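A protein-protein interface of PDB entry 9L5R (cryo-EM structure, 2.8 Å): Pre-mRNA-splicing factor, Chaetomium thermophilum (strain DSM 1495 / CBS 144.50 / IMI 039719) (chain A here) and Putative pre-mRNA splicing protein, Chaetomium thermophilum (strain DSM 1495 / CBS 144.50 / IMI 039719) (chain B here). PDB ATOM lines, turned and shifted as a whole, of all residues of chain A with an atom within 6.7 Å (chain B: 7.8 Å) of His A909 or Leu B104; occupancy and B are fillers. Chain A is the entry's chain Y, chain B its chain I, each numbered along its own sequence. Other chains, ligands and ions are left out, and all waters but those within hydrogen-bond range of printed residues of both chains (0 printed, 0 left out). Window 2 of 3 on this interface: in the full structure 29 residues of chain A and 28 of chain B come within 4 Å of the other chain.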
ATOM      1  N   LEU A 893      28.703  -8.690  -7.004  1.00  0.00           N
ATOM      2  CA  LEU A 893      27.637  -9.465  -7.628  1.00  0.00           C
ATOM      3  C   LEU A 893      26.754  -8.579  -8.497  1.00  0.00           C
ATOM      4  O   LEU A 893      26.306  -9.003  -9.569  1.00  0.00           O
ATOM      5  CB  LEU A 893      26.807 -10.178  -6.560  1.00  0.00           C
ATOM      6  CG  LEU A 893      27.329 -11.540  -6.096  1.00  0.00           C
ATOM      7  CD1 LEU A 893      26.319 -12.225  -5.187  1.00  0.00           C
ATOM      8  CD2 LEU A 893      27.676 -12.426  -7.284  1.00  0.00           C
ATOM      9  N   VAL A 896      28.795  -8.133 -11.604  1.00  0.00           N
ATOM     10  CA  VAL A 896      28.726  -9.316 -12.461  1.00  0.00           C
ATOM     11  C   VAL A 896      27.372  -9.396 -13.161  1.00  0.00           C
ATOM     12  O   VAL A 896      27.288  -9.791 -14.329  1.00  0.00           O
ATOM     13  CB  VAL A 896      29.037 -10.582 -11.637  1.00  0.00           C
ATOM     14  CG1 VAL A 896      28.712 -11.853 -12.411  1.00  0.00           C
ATOM     15  CG2 VAL A 896      30.501 -10.594 -11.258  1.00  0.00           C
ATOM     16  N   SER A 897      26.296  -9.008 -12.468  1.00  0.00           N
ATOM     17  CA  SER A 897      24.983  -8.949 -13.107  1.00  0.00           C
ATOM     18  C   SER A 897      24.960  -7.918 -14.232  1.00  0.00           C
ATOM     19  O   SER A 897      24.390  -8.168 -15.301  1.00  0.00           O
ATOM     20  CB  SER A 897      23.909  -8.634 -12.067  1.00  0.00           C
ATOM     21  OG  SER A 897      23.876  -9.622 -11.052  1.00  0.00           O
ATOM     22  N   ALA A 900      26.892  -9.432 -17.137  1.00  0.00           N
ATOM     23  CA  ALA A 900      26.091 -10.432 -17.835  1.00  0.00           C
ATOM     24  C   ALA A 900      25.001  -9.780 -18.676  1.00  0.00           C
ATOM     25  O   ALA A 900      24.698 -10.250 -19.780  1.00  0.00           O
ATOM     26  CB  ALA A 900      25.482 -11.411 -16.830  1.00  0.00           C
ATOM     27  N   ALA A 901      24.401  -8.698 -18.171  1.00  0.00           N
ATOM     28  CA  ALA A 901      23.420  -7.960 -18.961  1.00  0.00           C
ATOM     29  C   ALA A 901      24.059  -7.285 -20.168  1.00  0.00           C
ATOM     30  O   ALA A 901      23.433  -7.195 -21.230  1.00  0.00           O
ATOM     31  CB  ALA A 901      22.711  -6.926 -18.086  1.00  0.00           C
ATOM     32  N   ALA A 905      24.194 -12.656 -21.903  1.00  0.00           N
ATOM     33  CA  ALA A 905      24.101 -14.064 -21.549  1.00  0.00           C
ATOM     34  C   ALA A 905      22.778 -14.342 -20.838  1.00  0.00           C
ATOM     35  O   ALA A 905      22.292 -13.499 -20.078  1.00  0.00           O
ATOM     36  CB  ALA A 905      25.273 -14.467 -20.657  1.00  0.00           C
ATOM     37  N   PRO A 906      22.167 -15.504 -21.072  1.00  0.00           N
ATOM     38  CA  PRO A 906      20.898 -15.817 -20.405  1.00  0.00           C
ATOM     39  C   PRO A 906      21.078 -16.061 -18.914  1.00  0.00           C
ATOM     40  O   PRO A 906      22.130 -16.510 -18.453  1.00  0.00           O
ATOM     41  CB  PRO A 906      20.424 -17.086 -21.120  1.00  0.00           C
ATOM     42  CG  PRO A 906      21.669 -17.706 -21.651  1.00  0.00           C
ATOM     43  CD  PRO A 906      22.577 -16.565 -22.009  1.00  0.00           C
ATOM     44  N   GLY A 907      20.025 -15.755 -18.162  1.00  0.00           N
ATOM     45  CA  GLY A 907      20.012 -15.983 -16.733  1.00  0.00           C
ATOM     46  C   GLY A 907      20.686 -14.872 -15.950  1.00  0.00           C
ATOM     47  O   GLY A 907      21.368 -13.998 -16.489  1.00  0.00           O
ATOM     48  N   ALA A 908      20.485 -14.916 -14.634  1.00  0.00           N
ATOM     49  CA  ALA A 908      21.097 -13.971 -13.707  1.00  0.00           C
ATOM     50  C   ALA A 908      22.325 -14.637 -13.097  1.00  0.00           C
ATOM     51  O   ALA A 908      22.203 -15.499 -12.221  1.00  0.00           O
ATOM     52  CB  ALA A 908      20.106 -13.541 -12.627  1.00  0.00           C
ATOM     53  N   HIS A 909      23.504 -14.234 -13.561  1.00  0.00           N
ATOM     54  CA  HIS A 909      24.759 -14.849 -13.152  1.00  0.00           C
ATOM     55  C   HIS A 909      25.370 -14.195 -11.919  1.00  0.00           C
ATOM     56  O   HIS A 909      26.455 -14.605 -11.493  1.00  0.00           O
ATOM     57  CB  HIS A 909      25.754 -14.811 -14.312  1.00  0.00           C
ATOM     58  CG  HIS A 909      25.310 -15.594 -15.508  1.00  0.00           C
ATOM     59  ND1 HIS A 909      25.303 -16.971 -15.534  1.00  0.00           N
ATOM     60  CD2 HIS A 909      24.845 -15.191 -16.714  1.00  0.00           C
ATOM     61  CE1 HIS A 909      24.860 -17.385 -16.709  1.00  0.00           C
ATOM     62  NE2 HIS A 909      24.576 -16.324 -17.443  1.00  0.00           N
ATOM     63  N   GLY A 910      24.708 -13.196 -11.344  1.00  0.00           N
ATOM     64  CA  GLY A 910      25.184 -12.572 -10.126  1.00  0.00           C
ATOM     65  C   GLY A 910      24.512 -13.135  -8.891  1.00  0.00           C
ATOM     66  O   GLY A 910      24.345 -12.431  -7.890  1.00  0.00           O
ATOM     67  N   ASN A 911      24.106 -14.405  -8.961  1.00  0.00           N
ATOM     68  CA  ASN A 911      23.431 -15.040  -7.833  1.00  0.00           C
ATOM     69  C   ASN A 911      24.385 -15.255  -6.665  1.00  0.00           C
ATOM     70  O   ASN A 911      24.040 -14.978  -5.509  1.00  0.00           O
ATOM     71  CB  ASN A 911      22.814 -16.367  -8.274  1.00  0.00           C
ATOM     72  CG  ASN A 911      21.463 -16.192  -8.938  1.00  0.00           C
ATOM     73  OD1 ASN A 911      20.942 -15.080  -9.026  1.00  0.00           O
ATOM     74  ND2 ASN A 911      20.888 -17.293  -9.407  1.00  0.00           N
ATOM     75  N   SER A 912      25.590 -15.746  -6.943  1.00  0.00           N
ATOM     76  CA  SER A 912      26.565 -16.018  -5.897  1.00  0.00           C
ATOM     77  C   SER A 912      27.965 -15.914  -6.483  1.00  0.00           C
ATOM     78  O   SER A 912      28.147 -15.767  -7.695  1.00  0.00           O
ATOM     79  CB  SER A 912      26.339 -17.396  -5.264  1.00  0.00           C
ATOM     80  OG  SER A 912      26.857 -18.426  -6.087  1.00  0.00           O
ATOM     81  N   ALA A 913      28.959 -15.985  -5.593  1.00  0.00           N
ATOM     82  CA  ALA A 913      30.353 -15.868  -6.011  1.00  0.00           C
ATOM     83  C   ALA A 913      30.788 -17.055  -6.861  1.00  0.00           C
ATOM     84  O   ALA A 913      31.520 -16.885  -7.843  1.00  0.00           O
ATOM     85  CB  ALA A 913      31.254 -15.727  -4.785  1.00  0.00           C
ATOM     86  N   GLU A 914      30.356 -18.266  -6.494  1.00  0.00           N
ATOM     87  CA  GLU A 914      30.695 -19.450  -7.279  1.00  0.00           C
ATOM     88  C   GLU A 914      30.058 -19.399  -8.663  1.00  0.00           C
ATOM     89  O   GLU A 914      30.702 -19.748  -9.661  1.00  0.00           O
ATOM     90  CB  GLU A 914      30.262 -20.713  -6.534  1.00  0.00           C
ATOM     91  CG  GLU A 914      30.828 -22.001  -7.111  1.00  0.00           C
ATOM     92  CD  GLU A 914      30.242 -23.239  -6.459  1.00  0.00           C
ATOM     93  OE1 GLU A 914      29.552 -23.099  -5.428  1.00  0.00           O
ATOM     94  OE2 GLU A 914      30.473 -24.352  -6.978  1.00  0.00           O
ATOM     95  N   THR A 915      28.798 -18.957  -8.741  1.00  0.00           N
ATOM     96  CA  THR A 915      28.138 -18.805 -10.033  1.00  0.00           C
ATOM     97  C   THR A 915      28.811 -17.727 -10.874  1.00  0.00           C
ATOM     98  O   THR A 915      28.947 -17.880 -12.092  1.00  0.00           O
ATOM     99  CB  THR A 915      26.656 -18.481  -9.839  1.00  0.00           C
ATOM    100  OG1 THR A 915      26.523 -17.250  -9.115  1.00  0.00           O
ATOM    101  CG2 THR A 915      25.961 -19.597  -9.075  1.00  0.00           C
ATOM    102  N   ALA A 916      29.243 -16.633 -10.239  1.00  0.00           N
ATOM    103  CA  ALA A 916      29.952 -15.578 -10.960  1.00  0.00           C
ATOM    104  C   ALA A 916      31.289 -16.073 -11.501  1.00  0.00           C
ATOM    105  O   ALA A 916      31.648 -15.781 -12.648  1.00  0.00           O
ATOM    106  CB  ALA A 916      30.157 -14.368 -10.050  1.00  0.00           C
ATOM    107  N   GLY A 917      32.033 -16.833 -10.694  1.00  0.00           N
ATOM    108  CA  GLY A 917      33.302 -17.373 -11.158  1.00  0.00           C
ATOM    109  C   GLY A 917      33.138 -18.394 -12.268  1.00  0.00           C
ATOM    110  O   GLY A 917      33.932 -18.431 -13.215  1.00  0.00           O
ATOM    111  N   TYR A 918      32.106 -19.239 -12.171  1.00  0.00           N
ATOM    112  CA  TYR A 918      31.831 -20.193 -13.238  1.00  0.00           C
ATOM    113  C   TYR A 918      31.378 -19.496 -14.516  1.00  0.00           C
ATOM    114  O   TYR A 918      31.761 -19.916 -15.613  1.00  0.00           O
ATOM    115  CB  TYR A 918      30.789 -21.208 -12.773  1.00  0.00           C
ATOM    116  CG  TYR A 918      31.371 -22.332 -11.946  1.00  0.00           C
ATOM    117  CD1 TYR A 918      32.648 -22.816 -12.200  1.00  0.00           C
ATOM    118  CD2 TYR A 918      30.643 -22.912 -10.914  1.00  0.00           C
ATOM    119  CE1 TYR A 918      33.186 -23.845 -11.449  1.00  0.00           C
ATOM    120  CE2 TYR A 918      31.173 -23.942 -10.156  1.00  0.00           C
ATOM    121  CZ  TYR A 918      32.444 -24.404 -10.429  1.00  0.00           C
ATOM    122  OH  TYR A 918      32.975 -25.428  -9.678  1.00  0.00           O
ATOM    123  N   PHE A 919      30.580 -18.429 -14.391  1.00  0.00           N
ATOM    124  CA  PHE A 919      30.226 -17.606 -15.545  1.00  0.00           C
ATOM    125  C   PHE A 919      31.459 -16.983 -16.184  1.00  0.00           C
ATOM    126  O   PHE A 919      31.567 -16.930 -17.416  1.00  0.00           O
ATOM    127  CB  PHE A 919      29.236 -16.522 -15.119  1.00  0.00           C
ATOM    128  CG  PHE A 919      28.950 -15.505 -16.187  1.00  0.00           C
ATOM    129  CD1 PHE A 919      28.177 -15.829 -17.288  1.00  0.00           C
ATOM    130  CD2 PHE A 919      29.447 -14.214 -16.077  1.00  0.00           C
ATOM    131  CE1 PHE A 919      27.913 -14.885 -18.265  1.00  0.00           C
ATOM    132  CE2 PHE A 919      29.186 -13.269 -17.051  1.00  0.00           C
ATOM    133  CZ  PHE A 919      28.419 -13.606 -18.147  1.00  0.00           C
ATOM    134  N   TYR A 923      32.439 -17.934 -20.022  1.00  0.00           N
ATOM    135  CA  TYR A 923      32.261 -16.931 -21.069  1.00  0.00           C
ATOM    136  C   TYR A 923      33.510 -16.090 -21.320  1.00  0.00           C
ATOM    137  O   TYR A 923      33.981 -16.011 -22.458  1.00  0.00           O
ATOM    138  CB  TYR A 923      31.072 -16.025 -20.724  1.00  0.00           C
ATOM    139  CG  TYR A 923      29.737 -16.575 -21.170  1.00  0.00           C
ATOM    140  CD1 TYR A 923      29.006 -17.427 -20.351  1.00  0.00           C
ATOM    141  CD2 TYR A 923      29.206 -16.242 -22.410  1.00  0.00           C
ATOM    142  CE1 TYR A 923      27.784 -17.933 -20.754  1.00  0.00           C
ATOM    143  CE2 TYR A 923      27.984 -16.744 -22.823  1.00  0.00           C
ATOM    144  CZ  TYR A 923      27.278 -17.589 -21.991  1.00  0.00           C
ATOM    145  OH  TYR A 923      26.063 -18.090 -22.396  1.00  0.00           O
ATOM    146  N   CYS B  61      18.255 -27.451 -23.020  1.00  0.00           N
ATOM    147  CA  CYS B  61      19.120 -27.110 -21.897  1.00  0.00           C
ATOM    148  C   CYS B  61      19.959 -25.871 -22.185  1.00  0.00           C
ATOM    149  O   CYS B  61      20.333 -25.150 -21.254  1.00  0.00           O
ATOM    150  CB  CYS B  61      20.022 -28.294 -21.552  1.00  0.00           C
ATOM    151  SG  CYS B  61      19.148 -29.709 -20.843  1.00  0.00           S
ATOM    152  N   VAL B  62      20.278 -25.618 -23.456  1.00  0.00           N
ATOM    153  CA  VAL B  62      20.989 -24.394 -23.811  1.00  0.00           C
ATOM    154  C   VAL B  62      20.089 -23.177 -23.614  1.00  0.00           C
ATOM    155  O   VAL B  62      20.492 -22.179 -23.006  1.00  0.00           O
ATOM    156  CB  VAL B  62      21.523 -24.486 -25.254  1.00  0.00           C
ATOM    157  CG1 VAL B  62      21.789 -23.103 -25.836  1.00  0.00           C
ATOM    158  CG2 VAL B  62      22.793 -25.323 -25.293  1.00  0.00           C
ATOM    159  N   LEU B  64      17.084 -22.886 -21.902  1.00  0.00           N
ATOM    160  CA  LEU B  64      16.546 -22.751 -20.549  1.00  0.00           C
ATOM    161  C   LEU B  64      17.410 -23.582 -19.611  1.00  0.00           C
ATOM    162  O   LEU B  64      17.050 -24.711 -19.248  1.00  0.00           O
ATOM    163  CB  LEU B  64      15.081 -23.188 -20.487  1.00  0.00           C
ATOM    164  CG  LEU B  64      14.082 -22.371 -21.310  1.00  0.00           C
ATOM    165  CD1 LEU B  64      12.701 -23.009 -21.267  1.00  0.00           C
ATOM    166  CD2 LEU B  64      14.027 -20.933 -20.818  1.00  0.00           C
ATOM    167  N   PRO B  65      18.566 -23.054 -19.198  1.00  0.00           N
ATOM    168  CA  PRO B  65      19.464 -23.842 -18.340  1.00  0.00           C
ATOM    169  C   PRO B  65      18.988 -23.967 -16.904  1.00  0.00           C
ATOM    170  O   PRO B  65      19.471 -24.852 -16.187  1.00  0.00           O
ATOM    171  CB  PRO B  65      20.786 -23.072 -18.426  1.00  0.00           C
ATOM    172  CG  PRO B  65      20.360 -21.657 -18.636  1.00  0.00           C
ATOM    173  CD  PRO B  65      19.112 -21.715 -19.485  1.00  0.00           C
ATOM    174  N   ARG B  66      18.064 -23.119 -16.462  1.00  0.00           N
ATOM    175  CA  ARG B  66      17.498 -23.217 -15.124  1.00  0.00           C
ATOM    176  C   ARG B  66      16.344 -24.208 -15.046  1.00  0.00           C
ATOM    177  O   ARG B  66      15.776 -24.390 -13.964  1.00  0.00           O
ATOM    178  CB  ARG B  66      17.021 -21.843 -14.644  1.00  0.00           C
ATOM    179  CG  ARG B  66      18.140 -20.876 -14.296  1.00  0.00           C
ATOM    180  CD  ARG B  66      17.595 -19.623 -13.630  1.00  0.00           C
ATOM    181  NE  ARG B  66      18.662 -18.736 -13.181  1.00  0.00           N
ATOM    182  CZ  ARG B  66      18.469 -17.612 -12.503  1.00  0.00           C
ATOM    183  NH1 ARG B  66      17.254 -17.202 -12.176  1.00  0.00           N
ATOM    184  NH2 ARG B  66      19.520 -16.881 -12.145  1.00  0.00           N
ATOM    185  N   SER B  67      15.987 -24.844 -16.157  1.00  0.00           N
ATOM    186  CA  SER B  67      14.856 -25.769 -16.202  1.00  0.00           C
ATOM    187  C   SER B  67      15.328 -27.128 -15.700  1.00  0.00           C
ATOM    188  O   SER B  67      15.793 -27.970 -16.481  1.00  0.00           O
ATOM    189  CB  SER B  67      14.282 -25.851 -17.610  1.00  0.00           C
ATOM    190  OG  SER B  67      13.018 -26.485 -17.597  1.00  0.00           O
ATOM    191  N   PHE B  98      26.884 -32.598 -16.717  1.00  0.00           N
ATOM    192  CA  PHE B  98      26.661 -32.453 -15.282  1.00  0.00           C
ATOM    193  C   PHE B  98      27.367 -31.218 -14.734  1.00  0.00           C
ATOM    194  O   PHE B  98      26.842 -30.536 -13.848  1.00  0.00           O
ATOM    195  CB  PHE B  98      27.149 -33.703 -14.553  1.00  0.00           C
ATOM    196  CG  PHE B  98      26.078 -34.725 -14.296  1.00  0.00           C
ATOM    197  CD1 PHE B  98      25.142 -34.533 -13.292  1.00  0.00           C
ATOM    198  CD2 PHE B  98      26.020 -35.889 -15.046  1.00  0.00           C
ATOM    199  CE1 PHE B  98      24.165 -35.482 -13.045  1.00  0.00           C
ATOM    200  CE2 PHE B  98      25.043 -36.837 -14.809  1.00  0.00           C
ATOM    201  CZ  PHE B  98      24.113 -36.633 -13.808  1.00  0.00           C
ATOM    202  N   GLU B  99      28.564 -30.924 -15.248  1.00  0.00           N
ATOM    203  CA  GLU B  99      29.313 -29.755 -14.799  1.00  0.00           C
ATOM    204  C   GLU B  99      28.610 -28.461 -15.184  1.00  0.00           C
ATOM    205  O   GLU B  99      28.565 -27.524 -14.386  1.00  0.00           O
ATOM    206  CB  GLU B  99      30.731 -29.785 -15.366  1.00  0.00           C
ATOM    207  CG  GLU B  99      31.705 -30.630 -14.559  1.00  0.00           C
ATOM    208  CD  GLU B  99      32.112 -29.971 -13.256  1.00  0.00           C
ATOM    209  OE1 GLU B  99      32.016 -28.729 -13.158  1.00  0.00           O
ATOM    210  OE2 GLU B  99      32.528 -30.694 -12.327  1.00  0.00           O
ATOM    211  N   ARG B 100      28.056 -28.390 -16.397  1.00  0.00           N
ATOM    212  CA  ARG B 100      27.278 -27.213 -16.785  1.00  0.00           C
ATOM    213  C   ARG B 100      26.011 -27.084 -15.943  1.00  0.00           C
ATOM    214  O   ARG B 100      25.645 -25.976 -15.510  1.00  0.00           O
ATOM    215  CB  ARG B 100      26.927 -27.281 -18.272  1.00  0.00           C
ATOM    216  CG  ARG B 100      26.443 -25.963 -18.854  1.00  0.00           C
ATOM    217  CD  ARG B 100      25.998 -26.124 -20.298  1.00  0.00           C
ATOM    218  NE  ARG B 100      27.118 -26.379 -21.196  1.00  0.00           N
ATOM    219  CZ  ARG B 100      26.992 -26.723 -22.471  1.00  0.00           C
ATOM    220  NH1 ARG B 100      25.804 -26.862 -23.035  1.00  0.00           N
ATOM    221  NH2 ARG B 100      28.086 -26.933 -23.197  1.00  0.00           N
ATOM    222  N   ALA B 101      25.334 -28.211 -15.695  1.00  0.00           N
ATOM    223  CA  ALA B 101      24.113 -28.187 -14.897  1.00  0.00           C
ATOM    224  C   ALA B 101      24.386 -27.800 -13.450  1.00  0.00           C
ATOM    225  O   ALA B 101      23.520 -27.211 -12.802  1.00  0.00           O
ATOM    226  CB  ALA B 101      23.421 -29.545 -14.956  1.00  0.00           C
ATOM    227  N   LEU B 102      25.567 -28.121 -12.927  1.00  0.00           N
ATOM    228  CA  LEU B 102      25.949 -27.668 -11.595  1.00  0.00           C
ATOM    229  C   LEU B 102      26.562 -26.274 -11.594  1.00  0.00           C
ATOM    230  O   LEU B 102      26.622 -25.641 -10.537  1.00  0.00           O
ATOM    231  CB  LEU B 102      26.923 -28.657 -10.953  1.00  0.00           C
ATOM    232  CG  LEU B 102      26.261 -29.915 -10.388  1.00  0.00           C
ATOM    233  CD1 LEU B 102      27.305 -30.924  -9.950  1.00  0.00           C
ATOM    234  CD2 LEU B 102      25.339 -29.551  -9.235  1.00  0.00           C
ATOM    235  N   ILE B 103      27.044 -25.800 -12.744  1.00  0.00           N
ATOM    236  CA  ILE B 103      27.446 -24.403 -12.865  1.00  0.00           C
ATOM    237  C   ILE B 103      26.231 -23.498 -12.733  1.00  0.00           C
ATOM    238  O   ILE B 103      26.253 -22.501 -11.999  1.00  0.00           O
ATOM    239  CB  ILE B 103      28.193 -24.177 -14.197  1.00  0.00           C
ATOM    240  CG1 ILE B 103      29.675 -24.530 -14.050  1.00  0.00           C
ATOM    241  CG2 ILE B 103      28.038 -22.743 -14.700  1.00  0.00           C
ATOM    242  CD1 ILE B 103      30.408 -24.638 -15.368  1.00  0.00           C
ATOM    243  N   LEU B 104      25.141 -23.844 -13.414  1.00  0.00           N
ATOM    244  CA  LEU B 104      23.967 -22.979 -13.419  1.00  0.00           C
ATOM    245  C   LEU B 104      22.841 -23.458 -12.507  1.00  0.00           C
ATOM    246  O   LEU B 104      21.811 -22.783 -12.415  1.00  0.00           O
ATOM    247  CB  LEU B 104      23.454 -22.806 -14.851  1.00  0.00           C
ATOM    248  CG  LEU B 104      24.138 -21.628 -15.553  1.00  0.00           C
ATOM    249  CD1 LEU B 104      23.819 -21.588 -17.035  1.00  0.00           C
ATOM    250  CD2 LEU B 104      23.749 -20.317 -14.884  1.00  0.00           C
ATOM    251  N   LEU B 105      23.007 -24.594 -11.832  1.00  0.00           N
ATOM    252  CA  LEU B 105      22.000 -25.153 -10.930  1.00  0.00           C
ATOM    253  C   LEU B 105      22.677 -25.747  -9.695  1.00  0.00           C
ATOM    254  O   LEU B 105      22.407 -26.881  -9.297  1.00  0.00           O
ATOM    255  CB  LEU B 105      21.145 -26.202 -11.640  1.00  0.00           C
ATOM    256  CG  LEU B 105      20.142 -25.714 -12.690  1.00  0.00           C
ATOM    257  CD1 LEU B 105      19.488 -26.891 -13.398  1.00  0.00           C
ATOM    258  CD2 LEU B 105      19.092 -24.817 -12.052  1.00  0.00           C
ATOM    259  N   ASN B 106      23.585 -24.978  -9.085  1.00  0.00           N
ATOM    260  CA  ASN B 106      24.478 -25.501  -8.051  1.00  0.00           C
ATOM    261  C   ASN B 106      23.764 -25.926  -6.772  1.00  0.00           C
ATOM    262  O   ASN B 106      24.341 -26.682  -5.983  1.00  0.00           O
ATOM    263  CB  ASN B 106      25.543 -24.459  -7.704  1.00  0.00           C
ATOM    264  CG  ASN B 106      24.946 -23.105  -7.371  1.00  0.00           C
ATOM    265  OD1 ASN B 106      23.756 -22.870  -7.576  1.00  0.00           O
ATOM    266  ND2 ASN B 106      25.773 -22.207  -6.848  1.00  0.00           N
ATOM    267  N   LYS B 107      22.536 -25.467  -6.541  1.00  0.00           N
ATOM    268  CA  LYS B 107      21.849 -25.702  -5.279  1.00  0.00           C
ATOM    269  C   LYS B 107      20.882 -26.881  -5.326  1.00  0.00           C
ATOM    270  O   LYS B 107      19.893 -26.880  -4.584  1.00  0.00           O
ATOM    271  CB  LYS B 107      21.100 -24.438  -4.847  1.00  0.00           C
ATOM    272  CG  LYS B 107      21.999 -23.284  -4.444  1.00  0.00           C
ATOM    273  CD  LYS B 107      22.712 -23.567  -3.134  1.00  0.00           C
ATOM    274  CE  LYS B 107      23.409 -22.320  -2.615  1.00  0.00           C
ATOM    275  NZ  LYS B 107      23.901 -22.491  -1.221  1.00  0.00           N
ATOM    276  N   ILE B 111      20.664 -33.348  -8.184  1.00  0.00           N
ATOM    277  CA  ILE B 111      21.689 -33.291  -9.225  1.00  0.00           C
ATOM    278  C   ILE B 111      23.054 -33.638  -8.646  1.00  0.00           C
ATOM    279  O   ILE B 111      23.841 -34.368  -9.267  1.00  0.00           O
ATOM    280  CB  ILE B 111      21.692 -31.905  -9.898  1.00  0.00           C
ATOM    281  CG1 ILE B 111      20.361 -31.654 -10.605  1.00  0.00           C
ATOM    282  CG2 ILE B 111      22.835 -31.784 -10.898  1.00  0.00           C
ATOM    283  CD1 ILE B 111      20.299 -30.333 -11.345  1.00  0.00           C
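The guanidinium group (NH2) of Arg B66 sits close to the side-chain amide nitrogen (ND2) of Asn A911 (3.1 Å).
The guanidinium group (NH2) of Arg B66 is in hydrogen-bond range of the backbone carbonyl oxygen (O) of Ala A908.
His A909 touches Leu B104.
CG2 of Thr A915 touches ND2 of Asn B106, 3.4 Å away.
Ile B103 touches Tyr A918 (CG1 to CG, 3.5 Å).
Of the 17 printed residues of chain B, 4 touch a printed residue of chain A.
Printed residues of chain B that touch a printed residue of chain A: Arg B66, Ile B103, Leu B104 and Asn B106.
Of the 21 printed residues of chain A, 5 touch a printed residue of chain B.
Along chain A the printed residues that touch a printed residue of chain B span positions 908 to 918.
Among the printed residues, no Asp or Glu carboxylate lies within 4 Å of a Lys or Arg side-chain nitrogen of the other chain.
His A909 touches just one residue of chain B: Leu B104 (3.6 Å).
Of the printed residues of chain A, Leu B104 touches His A909 (3.6 Å).
Of chain B, only Arg B66 (3.0 Å) comes within 4 Å of Ala A908.
Of the printed residues of chain A, Arg B66 touches Ala A908 (3.0 Å) and Asn A911 (3.1 Å).
Printed residues of chain A within 4 Å of Ile B103: Tyr A918 (3.5 Å).
Of the printed residues of chain A, Asn B106 touches Thr A915 (3.4 Å).
Phe B98 touches none of the printed residues of chain A.
The nearest residue of chain B that does not touch His A909 is Arg B66 (5.0 Å).
The nearest printed residue of chain A that does not touch Asn B106 is Ser A912 (4.01 Å).
O of Ala A908 lies close to OD1 of Asn A911 (3.5 Å).
The backbone carbonyl oxygen of Pro A906 is in hydrogen-bond range of a ring nitrogen (NE2) of His A909, 2.7 Å away.
The side-chain hydroxyl (OG1) of Thr A915 sits at hydrogen-bond distance from the backbone carbonyl oxygen (O) of Ser A912.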
